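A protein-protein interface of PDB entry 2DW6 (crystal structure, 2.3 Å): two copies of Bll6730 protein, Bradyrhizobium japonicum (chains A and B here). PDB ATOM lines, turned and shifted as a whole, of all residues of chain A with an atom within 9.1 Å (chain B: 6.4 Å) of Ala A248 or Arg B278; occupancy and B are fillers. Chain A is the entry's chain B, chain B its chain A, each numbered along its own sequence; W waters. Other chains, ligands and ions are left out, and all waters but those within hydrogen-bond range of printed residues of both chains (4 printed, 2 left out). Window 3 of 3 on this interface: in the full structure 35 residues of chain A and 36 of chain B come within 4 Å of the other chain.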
ATOM      1  N   LEU A 220      15.050  22.014 -16.302  1.00  0.00           N
ATOM      2  CA  LEU A 220      15.929  21.034 -16.937  1.00  0.00           C
ATOM      3  C   LEU A 220      16.914  21.590 -17.966  1.00  0.00           C
ATOM      4  O   LEU A 220      18.114  21.324 -17.878  1.00  0.00           O
ATOM      5  CB  LEU A 220      15.121  19.912 -17.590  1.00  0.00           C
ATOM      6  CG  LEU A 220      15.992  18.832 -18.246  1.00  0.00           C
ATOM      7  CD1 LEU A 220      16.946  18.222 -17.222  1.00  0.00           C
ATOM      8  CD2 LEU A 220      15.102  17.760 -18.849  1.00  0.00           C
ATOM      9  N   ILE A 224      21.030  21.861 -17.620  1.00  0.00           N
ATOM     10  CA  ILE A 224      21.940  21.225 -18.567  1.00  0.00           C
ATOM     11  C   ILE A 224      22.905  22.240 -19.170  1.00  0.00           C
ATOM     12  O   ILE A 224      24.091  21.957 -19.345  1.00  0.00           O
ATOM     13  CB  ILE A 224      21.158  20.526 -19.704  1.00  0.00           C
ATOM     14  CG1 ILE A 224      20.369  19.342 -19.131  1.00  0.00           C
ATOM     15  CG2 ILE A 224      22.123  20.047 -20.784  1.00  0.00           C
ATOM     16  CD1 ILE A 224      19.525  18.599 -20.146  1.00  0.00           C
ATOM     17  N   GLY A 242      18.077  21.910  -9.680  1.00  0.00           N
ATOM     18  CA  GLY A 242      16.681  22.240  -9.900  1.00  0.00           C
ATOM     19  C   GLY A 242      15.862  22.131  -8.635  1.00  0.00           C
ATOM     20  O   GLY A 242      16.407  21.887  -7.559  1.00  0.00           O
ATOM     21  N   ASP A 243      14.551  22.309  -8.769  1.00  0.00           N
ATOM     22  CA  ASP A 243      13.638  22.242  -7.636  1.00  0.00           C
ATOM     23  C   ASP A 243      13.971  21.012  -6.798  1.00  0.00           C
ATOM     24  O   ASP A 243      14.126  19.915  -7.330  1.00  0.00           O
ATOM     25  CB  ASP A 243      12.190  22.193  -8.139  1.00  0.00           C
ATOM     26  CG  ASP A 243      11.177  22.282  -7.013  1.00  0.00           C
ATOM     27  OD1 ASP A 243      10.984  21.274  -6.295  1.00  0.00           O
ATOM     28  OD2 ASP A 243      10.578  23.364  -6.838  1.00  0.00           O
ATOM     29  N   PRO A 244      14.090  21.180  -5.470  1.00  0.00           N
ATOM     30  CA  PRO A 244      14.422  20.066  -4.569  1.00  0.00           C
ATOM     31  C   PRO A 244      13.514  18.837  -4.662  1.00  0.00           C
ATOM     32  O   PRO A 244      13.912  17.731  -4.270  1.00  0.00           O
ATOM     33  CB  PRO A 244      14.399  20.723  -3.184  1.00  0.00           C
ATOM     34  CG  PRO A 244      13.425  21.844  -3.356  1.00  0.00           C
ATOM     35  CD  PRO A 244      13.788  22.401  -4.703  1.00  0.00           C
ATOM     36  N   LEU A 245      12.310  19.022  -5.194  1.00  0.00           N
ATOM     37  CA  LEU A 245      11.362  17.918  -5.328  1.00  0.00           C
ATOM     38  C   LEU A 245      11.249  17.324  -6.739  1.00  0.00           C
ATOM     39  O   LEU A 245      10.550  16.324  -6.943  1.00  0.00           O
ATOM     40  CB  LEU A 245       9.982  18.361  -4.839  1.00  0.00           C
ATOM     41  CG  LEU A 245       9.885  18.607  -3.331  1.00  0.00           C
ATOM     42  CD1 LEU A 245       8.560  19.269  -3.018  1.00  0.00           C
ATOM     43  CD2 LEU A 245      10.029  17.290  -2.579  1.00  0.00           C
ATOM     44  N   ASP A 246      11.932  17.930  -7.712  1.00  0.00           N
ATOM     45  CA  ASP A 246      11.899  17.423  -9.089  1.00  0.00           C
ATOM     46  C   ASP A 246      13.019  16.394  -9.237  1.00  0.00           C
ATOM     47  O   ASP A 246      14.083  16.677  -9.803  1.00  0.00           O
ATOM     48  CB  ASP A 246      12.110  18.559 -10.095  1.00  0.00           C
ATOM     49  CG  ASP A 246      11.795  18.139 -11.524  1.00  0.00           C
ATOM     50  OD1 ASP A 246      11.746  16.912 -11.791  1.00  0.00           O
ATOM     51  OD2 ASP A 246      11.604  19.037 -12.382  1.00  0.00           O
ATOM     52  N   TYR A 247      12.772  15.199  -8.716  1.00  0.00           N
ATOM     53  CA  TYR A 247      13.751  14.130  -8.749  1.00  0.00           C
ATOM     54  C   TYR A 247      14.123  13.718 -10.167  1.00  0.00           C
ATOM     55  O   TYR A 247      15.276  13.375 -10.436  1.00  0.00           O
ATOM     56  CB  TYR A 247      13.223  12.924  -7.966  1.00  0.00           C
ATOM     57  CG  TYR A 247      12.801  13.270  -6.552  1.00  0.00           C
ATOM     58  CD1 TYR A 247      13.678  13.924  -5.684  1.00  0.00           C
ATOM     59  CD2 TYR A 247      11.526  12.946  -6.079  1.00  0.00           C
ATOM     60  CE1 TYR A 247      13.300  14.245  -4.386  1.00  0.00           C
ATOM     61  CE2 TYR A 247      11.138  13.262  -4.776  1.00  0.00           C
ATOM     62  CZ  TYR A 247      12.032  13.908  -3.934  1.00  0.00           C
ATOM     63  OH  TYR A 247      11.666  14.194  -2.637  1.00  0.00           O
ATOM     64  N   ALA A 248      13.151  13.761 -11.072  1.00  0.00           N
ATOM     65  CA  ALA A 248      13.405  13.382 -12.454  1.00  0.00           C
ATOM     66  C   ALA A 248      14.435  14.317 -13.084  1.00  0.00           C
ATOM     67  O   ALA A 248      15.277  13.883 -13.869  1.00  0.00           O
ATOM     68  CB  ALA A 248      12.103  13.398 -13.248  1.00  0.00           C
ATOM     69  N   LEU A 249      14.377  15.598 -12.737  1.00  0.00           N
ATOM     70  CA  LEU A 249      15.335  16.552 -13.286  1.00  0.00           C
ATOM     71  C   LEU A 249      16.745  16.178 -12.829  1.00  0.00           C
ATOM     72  O   LEU A 249      17.674  16.119 -13.633  1.00  0.00           O
ATOM     73  CB  LEU A 249      14.988  17.980 -12.845  1.00  0.00           C
ATOM     74  CG  LEU A 249      15.857  19.117 -13.409  1.00  0.00           C
ATOM     75  CD1 LEU A 249      15.107  20.441 -13.325  1.00  0.00           C
ATOM     76  CD2 LEU A 249      17.183  19.195 -12.643  1.00  0.00           C
ATOM     77  N   GLN A 250      16.897  15.914 -11.534  1.00  0.00           N
ATOM     78  CA  GLN A 250      18.191  15.533 -10.985  1.00  0.00           C
ATOM     79  C   GLN A 250      18.737  14.278 -11.676  1.00  0.00           C
ATOM     80  O   GLN A 250      19.909  14.222 -12.046  1.00  0.00           O
ATOM     81  CB  GLN A 250      18.068  15.280  -9.480  1.00  0.00           C
ATOM     82  CG  GLN A 250      19.378  14.846  -8.827  1.00  0.00           C
ATOM     83  CD  GLN A 250      20.471  15.887  -8.976  1.00  0.00           C
ATOM     84  OE1 GLN A 250      21.651  15.555  -9.105  1.00  0.00           O
ATOM     85  NE2 GLN A 250      20.083  17.156  -8.955  1.00  0.00           N
ATOM     86  N   ALA A 251      17.882  13.272 -11.841  1.00  0.00           N
ATOM     87  CA  ALA A 251      18.277  12.024 -12.481  1.00  0.00           C
ATOM     88  C   ALA A 251      18.812  12.252 -13.893  1.00  0.00           C
ATOM     89  O   ALA A 251      19.820  11.664 -14.299  1.00  0.00           O
ATOM     90  CB  ALA A 251      17.091  11.063 -12.523  1.00  0.00           C
ATOM     91  N   ALA A 252      18.130  13.109 -14.639  1.00  0.00           N
ATOM     92  CA  ALA A 252      18.521  13.404 -16.004  1.00  0.00           C
ATOM     93  C   ALA A 252      19.873  14.121 -16.116  1.00  0.00           C
ATOM     94  O   ALA A 252      20.534  14.063 -17.154  1.00  0.00           O
ATOM     95  CB  ALA A 252      17.431  14.233 -16.671  1.00  0.00           C
ATOM     96  N   LEU A 253      20.292  14.788 -15.049  1.00  0.00           N
ATOM     97  CA  LEU A 253      21.554  15.516 -15.078  1.00  0.00           C
ATOM     98  C   LEU A 253      22.790  14.630 -15.113  1.00  0.00           C
ATOM     99  O   LEU A 253      23.834  15.032 -15.623  1.00  0.00           O
ATOM    100  CB  LEU A 253      21.635  16.470 -13.884  1.00  0.00           C
ATOM    101  CG  LEU A 253      21.295  17.933 -14.171  1.00  0.00           C
ATOM    102  CD1 LEU A 253      20.066  18.067 -15.047  1.00  0.00           C
ATOM    103  CD2 LEU A 253      21.080  18.621 -12.842  1.00  0.00           C
ATOM    104  N   ALA A 254      22.674  13.424 -14.573  1.00  0.00           N
ATOM    105  CA  ALA A 254      23.803  12.498 -14.558  1.00  0.00           C
ATOM    106  C   ALA A 254      24.393  12.298 -15.959  1.00  0.00           C
ATOM    107  O   ALA A 254      25.592  12.074 -16.106  1.00  0.00           O
ATOM    108  CB  ALA A 254      23.366  11.151 -13.972  1.00  0.00           C
ATOM    109  N   GLU A 255      23.547  12.391 -16.981  1.00  0.00           N
ATOM    110  CA  GLU A 255      23.976  12.213 -18.368  1.00  0.00           C
ATOM    111  C   GLU A 255      24.905  13.329 -18.864  1.00  0.00           C
ATOM    112  O   GLU A 255      25.739  13.113 -19.749  1.00  0.00           O
ATOM    113  CB  GLU A 255      22.746  12.146 -19.289  1.00  0.00           C
ATOM    114  CG  GLU A 255      23.070  11.853 -20.755  1.00  0.00           C
ATOM    115  CD  GLU A 255      21.879  12.029 -21.704  1.00  0.00           C
ATOM    116  OE1 GLU A 255      20.723  11.782 -21.289  1.00  0.00           O
ATOM    117  OE2 GLU A 255      22.114  12.399 -22.878  1.00  0.00           O
ATOM    118  N   ASN A 275      12.534   9.499  -0.941  1.00  0.00           N
ATOM    119  CA  ASN A 275      12.154   9.737  -2.325  1.00  0.00           C
ATOM    120  C   ASN A 275      13.333  10.243  -3.151  1.00  0.00           C
ATOM    121  O   ASN A 275      13.447   9.923  -4.336  1.00  0.00           O
ATOM    122  CB  ASN A 275      10.975  10.714  -2.402  1.00  0.00           C
ATOM    123  CG  ASN A 275       9.672  10.089  -1.923  1.00  0.00           C
ATOM    124  OD1 ASN A 275       9.521   8.868  -1.937  1.00  0.00           O
ATOM    125  ND2 ASN A 275       8.723  10.923  -1.510  1.00  0.00           N
ATOM    126  N   LEU A 276      14.216  11.026  -2.535  1.00  0.00           N
ATOM    127  CA  LEU A 276      15.395  11.514  -3.252  1.00  0.00           C
ATOM    128  C   LEU A 276      16.276  10.325  -3.626  1.00  0.00           C
ATOM    129  O   LEU A 276      16.767  10.232  -4.754  1.00  0.00           O
ATOM    130  CB  LEU A 276      16.214  12.485  -2.391  1.00  0.00           C
ATOM    131  CG  LEU A 276      17.561  12.882  -3.019  1.00  0.00           C
ATOM    132  CD1 LEU A 276      17.336  13.704  -4.285  1.00  0.00           C
ATOM    133  CD2 LEU A 276      18.374  13.688  -2.022  1.00  0.00           C
ATOM    134  N   ARG A 278      15.328   7.209  -3.926  1.00  0.00           N
ATOM    135  CA  ARG A 278      14.570   6.337  -4.826  1.00  0.00           C
ATOM    136  C   ARG A 278      14.492   6.844  -6.261  1.00  0.00           C
ATOM    137  O   ARG A 278      14.691   6.074  -7.196  1.00  0.00           O
ATOM    138  CB  ARG A 278      13.125   6.137  -4.319  1.00  0.00           C
ATOM    139  CG  ARG A 278      12.950   5.079  -3.233  1.00  0.00           C
ATOM    140  CD  ARG A 278      11.520   5.061  -2.687  1.00  0.00           C
ATOM    141  NE  ARG A 278      11.305   3.941  -1.768  1.00  0.00           N
ATOM    142  CZ  ARG A 278      10.244   3.812  -0.972  1.00  0.00           C
ATOM    143  NH1 ARG A 278      10.131   2.758  -0.173  1.00  0.00           N
ATOM    144  NH2 ARG A 278       9.302   4.745  -0.957  1.00  0.00           N
ATOM    145  N   TYR A 279      14.229   8.135  -6.438  1.00  0.00           N
ATOM    146  CA  TYR A 279      14.049   8.671  -7.786  1.00  0.00           C
ATOM    147  C   TYR A 279      15.026   9.723  -8.292  1.00  0.00           C
ATOM    148  O   TYR A 279      14.981  10.086  -9.470  1.00  0.00           O
ATOM    149  CB  TYR A 279      12.629   9.232  -7.900  1.00  0.00           C
ATOM    150  CG  TYR A 279      11.587   8.376  -7.210  1.00  0.00           C
ATOM    151  CD1 TYR A 279      11.254   7.110  -7.697  1.00  0.00           C
ATOM    152  CD2 TYR A 279      10.942   8.827  -6.060  1.00  0.00           C
ATOM    153  CE1 TYR A 279      10.299   6.314  -7.048  1.00  0.00           C
ATOM    154  CE2 TYR A 279       9.996   8.049  -5.409  1.00  0.00           C
ATOM    155  CZ  TYR A 279       9.674   6.795  -5.901  1.00  0.00           C
ATOM    156  OH  TYR A 279       8.727   6.031  -5.237  1.00  0.00           O
ATOM    157  N   GLY A 280      15.903  10.207  -7.418  1.00  0.00           N
ATOM    158  CA  GLY A 280      16.853  11.242  -7.800  1.00  0.00           C
ATOM    159  C   GLY A 280      17.978  10.851  -8.740  1.00  0.00           C
ATOM    160  O   GLY A 280      18.551  11.713  -9.409  1.00  0.00           O
ATOM    161  N   GLY A 281      18.306   9.563  -8.788  1.00  0.00           N
ATOM    162  CA  GLY A 281      19.373   9.107  -9.658  1.00  0.00           C
ATOM    163  C   GLY A 281      20.738   9.659  -9.290  1.00  0.00           C
ATOM    164  O   GLY A 281      21.561   9.938 -10.160  1.00  0.00           O
ATOM    165  N   GLN B 271       4.430  20.421  -7.198  1.00  0.00           N
ATOM    166  CA  GLN B 271       5.617  19.563  -7.260  1.00  0.00           C
ATOM    167  C   GLN B 271       5.319  18.221  -6.598  1.00  0.00           C
ATOM    168  O   GLN B 271       5.666  17.167  -7.135  1.00  0.00           O
ATOM    169  CB  GLN B 271       6.826  20.196  -6.554  1.00  0.00           C
ATOM    170  CG  GLN B 271       7.411  21.404  -7.262  1.00  0.00           C
ATOM    171  CD  GLN B 271       6.825  22.701  -6.762  1.00  0.00           C
ATOM    172  OE1 GLN B 271       5.640  22.774  -6.420  1.00  0.00           O
ATOM    173  NE2 GLN B 271       7.648  23.740  -6.726  1.00  0.00           N
ATOM    174  N   ALA B 273       2.337  16.946  -6.108  1.00  0.00           N
ATOM    175  CA  ALA B 273       1.298  16.285  -6.890  1.00  0.00           C
ATOM    176  C   ALA B 273       1.950  15.616  -8.095  1.00  0.00           C
ATOM    177  O   ALA B 273       1.597  14.491  -8.459  1.00  0.00           O
ATOM    178  CB  ALA B 273       0.254  17.293  -7.343  1.00  0.00           C
ATOM    179  N   ARG B 274       2.911  16.305  -8.704  1.00  0.00           N
ATOM    180  CA  ARG B 274       3.618  15.751  -9.852  1.00  0.00           C
ATOM    181  C   ARG B 274       4.291  14.431  -9.459  1.00  0.00           C
ATOM    182  O   ARG B 274       4.242  13.450 -10.207  1.00  0.00           O
ATOM    183  CB  ARG B 274       4.664  16.747 -10.365  1.00  0.00           C
ATOM    184  CG  ARG B 274       5.399  16.305 -11.627  1.00  0.00           C
ATOM    185  CD  ARG B 274       6.166  17.473 -12.221  1.00  0.00           C
ATOM    186  NE  ARG B 274       7.110  18.030 -11.257  1.00  0.00           N
ATOM    187  CZ  ARG B 274       7.524  19.293 -11.259  1.00  0.00           C
ATOM    188  NH1 ARG B 274       7.082  20.141 -12.175  1.00  0.00           N
ATOM    189  NH2 ARG B 274       8.375  19.713 -10.333  1.00  0.00           N
ATOM    190  N   ASN B 275       4.916  14.401  -8.286  1.00  0.00           N
ATOM    191  CA  ASN B 275       5.574  13.180  -7.832  1.00  0.00           C
ATOM    192  C   ASN B 275       4.568  12.053  -7.589  1.00  0.00           C
ATOM    193  O   ASN B 275       4.876  10.884  -7.825  1.00  0.00           O
ATOM    194  CB  ASN B 275       6.406  13.442  -6.568  1.00  0.00           C
ATOM    195  CG  ASN B 275       7.654  14.262  -6.860  1.00  0.00           C
ATOM    196  OD1 ASN B 275       8.162  14.254  -7.984  1.00  0.00           O
ATOM    197  ND2 ASN B 275       8.160  14.964  -5.849  1.00  0.00           N
ATOM    198  N   LEU B 276       3.368  12.396  -7.126  1.00  0.00           N
ATOM    199  CA  LEU B 276       2.350  11.377  -6.914  1.00  0.00           C
ATOM    200  C   LEU B 276       1.993  10.754  -8.268  1.00  0.00           C
ATOM    201  O   LEU B 276       1.910   9.536  -8.391  1.00  0.00           O
ATOM    202  CB  LEU B 276       1.088  11.974  -6.291  1.00  0.00           C
ATOM    203  CG  LEU B 276      -0.105  11.006  -6.229  1.00  0.00           C
ATOM    204  CD1 LEU B 276       0.208   9.863  -5.277  1.00  0.00           C
ATOM    205  CD2 LEU B 276      -1.353  11.744  -5.764  1.00  0.00           C
ATOM    206  N   LEU B 277       1.799  11.590  -9.286  1.00  0.00           N
ATOM    207  CA  LEU B 277       1.440  11.080 -10.609  1.00  0.00           C
ATOM    208  C   LEU B 277       2.585  10.299 -11.259  1.00  0.00           C
ATOM    209  O   LEU B 277       2.362   9.328 -11.980  1.00  0.00           O
ATOM    210  CB  LEU B 277       0.985  12.235 -11.525  1.00  0.00           C
ATOM    211  CG  LEU B 277      -0.274  12.981 -11.064  1.00  0.00           C
ATOM    212  CD1 LEU B 277      -0.767  13.929 -12.152  1.00  0.00           C
ATOM    213  CD2 LEU B 277      -1.353  11.971 -10.720  1.00  0.00           C
ATOM    214  N   ARG B 278       3.815  10.718 -10.988  1.00  0.00           N
ATOM    215  CA  ARG B 278       4.989  10.052 -11.534  1.00  0.00           C
ATOM    216  C   ARG B 278       5.301   8.704 -10.891  1.00  0.00           C
ATOM    217  O   ARG B 278       5.605   7.743 -11.592  1.00  0.00           O
ATOM    218  CB  ARG B 278       6.238  10.939 -11.387  1.00  0.00           C
ATOM    219  CG  ARG B 278       6.396  12.028 -12.442  1.00  0.00           C
ATOM    220  CD  ARG B 278       7.584  12.947 -12.133  1.00  0.00           C
ATOM    221  NE  ARG B 278       7.844  13.887 -13.223  1.00  0.00           N
ATOM    222  CZ  ARG B 278       8.651  14.941 -13.133  1.00  0.00           C
ATOM    223  NH1 ARG B 278       8.829  15.737 -14.181  1.00  0.00           N
ATOM    224  NH2 ARG B 278       9.274  15.218 -11.990  1.00  0.00           N
ATOM    225  N   TYR B 279       5.213   8.620  -9.563  1.00  0.00           N
ATOM    226  CA  TYR B 279       5.596   7.383  -8.876  1.00  0.00           C
ATOM    227  C   TYR B 279       4.537   6.631  -8.078  1.00  0.00           C
ATOM    228  O   TYR B 279       4.797   5.522  -7.597  1.00  0.00           O
ATOM    229  CB  TYR B 279       6.776   7.687  -7.947  1.00  0.00           C
ATOM    230  CG  TYR B 279       7.805   8.629  -8.541  1.00  0.00           C
ATOM    231  CD1 TYR B 279       8.602   8.241  -9.621  1.00  0.00           C
ATOM    232  CD2 TYR B 279       7.964   9.922  -8.038  1.00  0.00           C
ATOM    233  CE1 TYR B 279       9.532   9.121 -10.184  1.00  0.00           C
ATOM    234  CE2 TYR B 279       8.881  10.806  -8.593  1.00  0.00           C
ATOM    235  CZ  TYR B 279       9.662  10.405  -9.663  1.00  0.00           C
ATOM    236  OH  TYR B 279      10.566  11.281 -10.224  1.00  0.00           O
ATOM    237  N   GLY B 280       3.356   7.219  -7.936  1.00  0.00           N
ATOM    238  CA  GLY B 280       2.305   6.587  -7.155  1.00  0.00           C
ATOM    239  C   GLY B 280       1.633   5.367  -7.755  1.00  0.00           C
ATOM    240  O   GLY B 280       1.057   4.564  -7.027  1.00  0.00           O
ATOM    241  N   GLY B 281       1.695   5.228  -9.076  1.00  0.00           N
ATOM    242  CA  GLY B 281       1.080   4.086  -9.727  1.00  0.00           C
ATOM    243  C   GLY B 281      -0.433   4.058  -9.594  1.00  0.00           C
ATOM    244  O   GLY B 281      -1.031   2.989  -9.480  1.00  0.00           O
ATOM    245  N   HIS B 312       0.371  14.683 -17.454  1.00  0.00           N
ATOM    246  CA  HIS B 312       0.437  13.252 -17.180  1.00  0.00           C
ATOM    247  C   HIS B 312      -0.780  12.472 -17.670  1.00  0.00           C
ATOM    248  O   HIS B 312      -0.981  11.324 -17.286  1.00  0.00           O
ATOM    249  CB  HIS B 312       0.655  13.026 -15.683  1.00  0.00           C
ATOM    250  CG  HIS B 312       2.009  13.457 -15.215  1.00  0.00           C
ATOM    251  ND1 HIS B 312       3.043  12.567 -15.010  1.00  0.00           N
ATOM    252  CD2 HIS B 312       2.531  14.693 -15.013  1.00  0.00           C
ATOM    253  CE1 HIS B 312       4.142  13.238 -14.708  1.00  0.00           C
ATOM    254  NE2 HIS B 312       3.859  14.529 -14.706  1.00  0.00           N
HETATM  255  O   HOH W   1      12.919  10.088 -11.236  1.00  0.00           O
HETATM  256  O   HOH W   2      10.493  18.211 -14.922  1.00  0.00           O
HETATM  257  O   HOH W   3       7.364   4.284  -6.949  1.00  0.00           O
HETATM  258  O   HOH W   4       9.367  23.418  -4.420  1.00  0.00           O
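NE2 of Gln B271 is in hydrogen-bond range of OD2 of Asp A243 (3.0 Å).
NH2 of Arg B278 is in salt-bridge range of OD1 of Asp A246.
The side-chain carboxylate of Asp A246 lies within salt-bridge range of the guanidinium group of Arg B274 (3.9 Å).
O of Leu A245 is in hydrogen-bond range of ND2 of Asn B275 (3.0 Å).
The backbone NH of Leu A249 is in hydrogen-bond range of the side-chain carboxylate of Asp A246, at 3.1 Å.
OD1 of Asp A243 lies within hydrogen-bond range of N of Leu A245.
Among the printed residues, pairs that only touch across the chains: Tyr A247 with Asn B275 (3.6 Å), Tyr A247 with Tyr B279 (3.9 Å), Ala A248 with Arg B278 (3.6 Å), Ala A248 with Tyr B279 (3.7 Å) and Tyr A279 with Tyr B279 (3.5 Å).
Ala A248 touches just these residues of chain B: Arg B278 (3.6 Å) and Tyr B279 (3.7 Å).
Arg B278 touches two residues of chain A.
Tyr B279 touches just these residues of chain A: Tyr A247, Ala A248 and Tyr A279.
Of the printed residues of chain B, Asp A243 touches Gln B271.
Of the printed residues of chain B, Asp A246 touches Arg B274 (3.9 Å) and Arg B278 (3.0 Å).
Of the printed residues of chain B, Tyr A279 touches Tyr B279 (3.5 Å).
Printed residues of chain A within 4 Å of Arg B274: Asp A246 (3.9 Å).
Of the printed residues of chain B, Leu A245 touches Asn B275.
Leu A220 touches none of the printed residues of chain B.
Ala B273 touches none of the printed residues of chain A.
The nearest residue of chain B that does not touch Ala A248 is Asn B275 (5.9 Å).
The nearest residue of chain A that does not touch Arg B278 is Tyr A247 (4.8 Å).
Printed residues of chain B that touch a printed residue of chain A: Gln B271, Arg B274, Asn B275, Arg B278 and Tyr B279.
Printed residues of chain A that touch a printed residue of chain B: Asp A243, Leu A245, Asp A246, Tyr A247, Ala A248 and Tyr A279.
Hydrophobic or aromatic side chains of chain A within 4 Å of the printed part of chain B: Leu A245, Tyr A247, Ala A248 and Tyr A279.
Among the printed residues, Asp or Glu carboxylates within 4 Å of a Lys or Arg side-chain nitrogen of the other chain: Asp A246 with Arg B274 (3.9 Å) and Asp A246 with Arg B278 (3.0 Å).
Tyr A279 touches its own counterpart, Tyr B279.
Of the 9 pairs that touch across the chains among the printed residues, 1 has its exchanged pair printed and touching as well.
Water W4 lies within hydrogen-bond range of OD2 of Asp A243 and NE2 of Gln B271.
Water W1 bridges O of Tyr A279 (2.7 Å) and OH of Tyr B279 (2.8 Å).
Water W3 bridges OH of Tyr A279 (2.8 Å) and O of Tyr B279 (2.9 Å).
Water W2 bridges OD2 of Asp A246 (2.9 Å) and NH1 of Arg B278 (3.1 Å).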
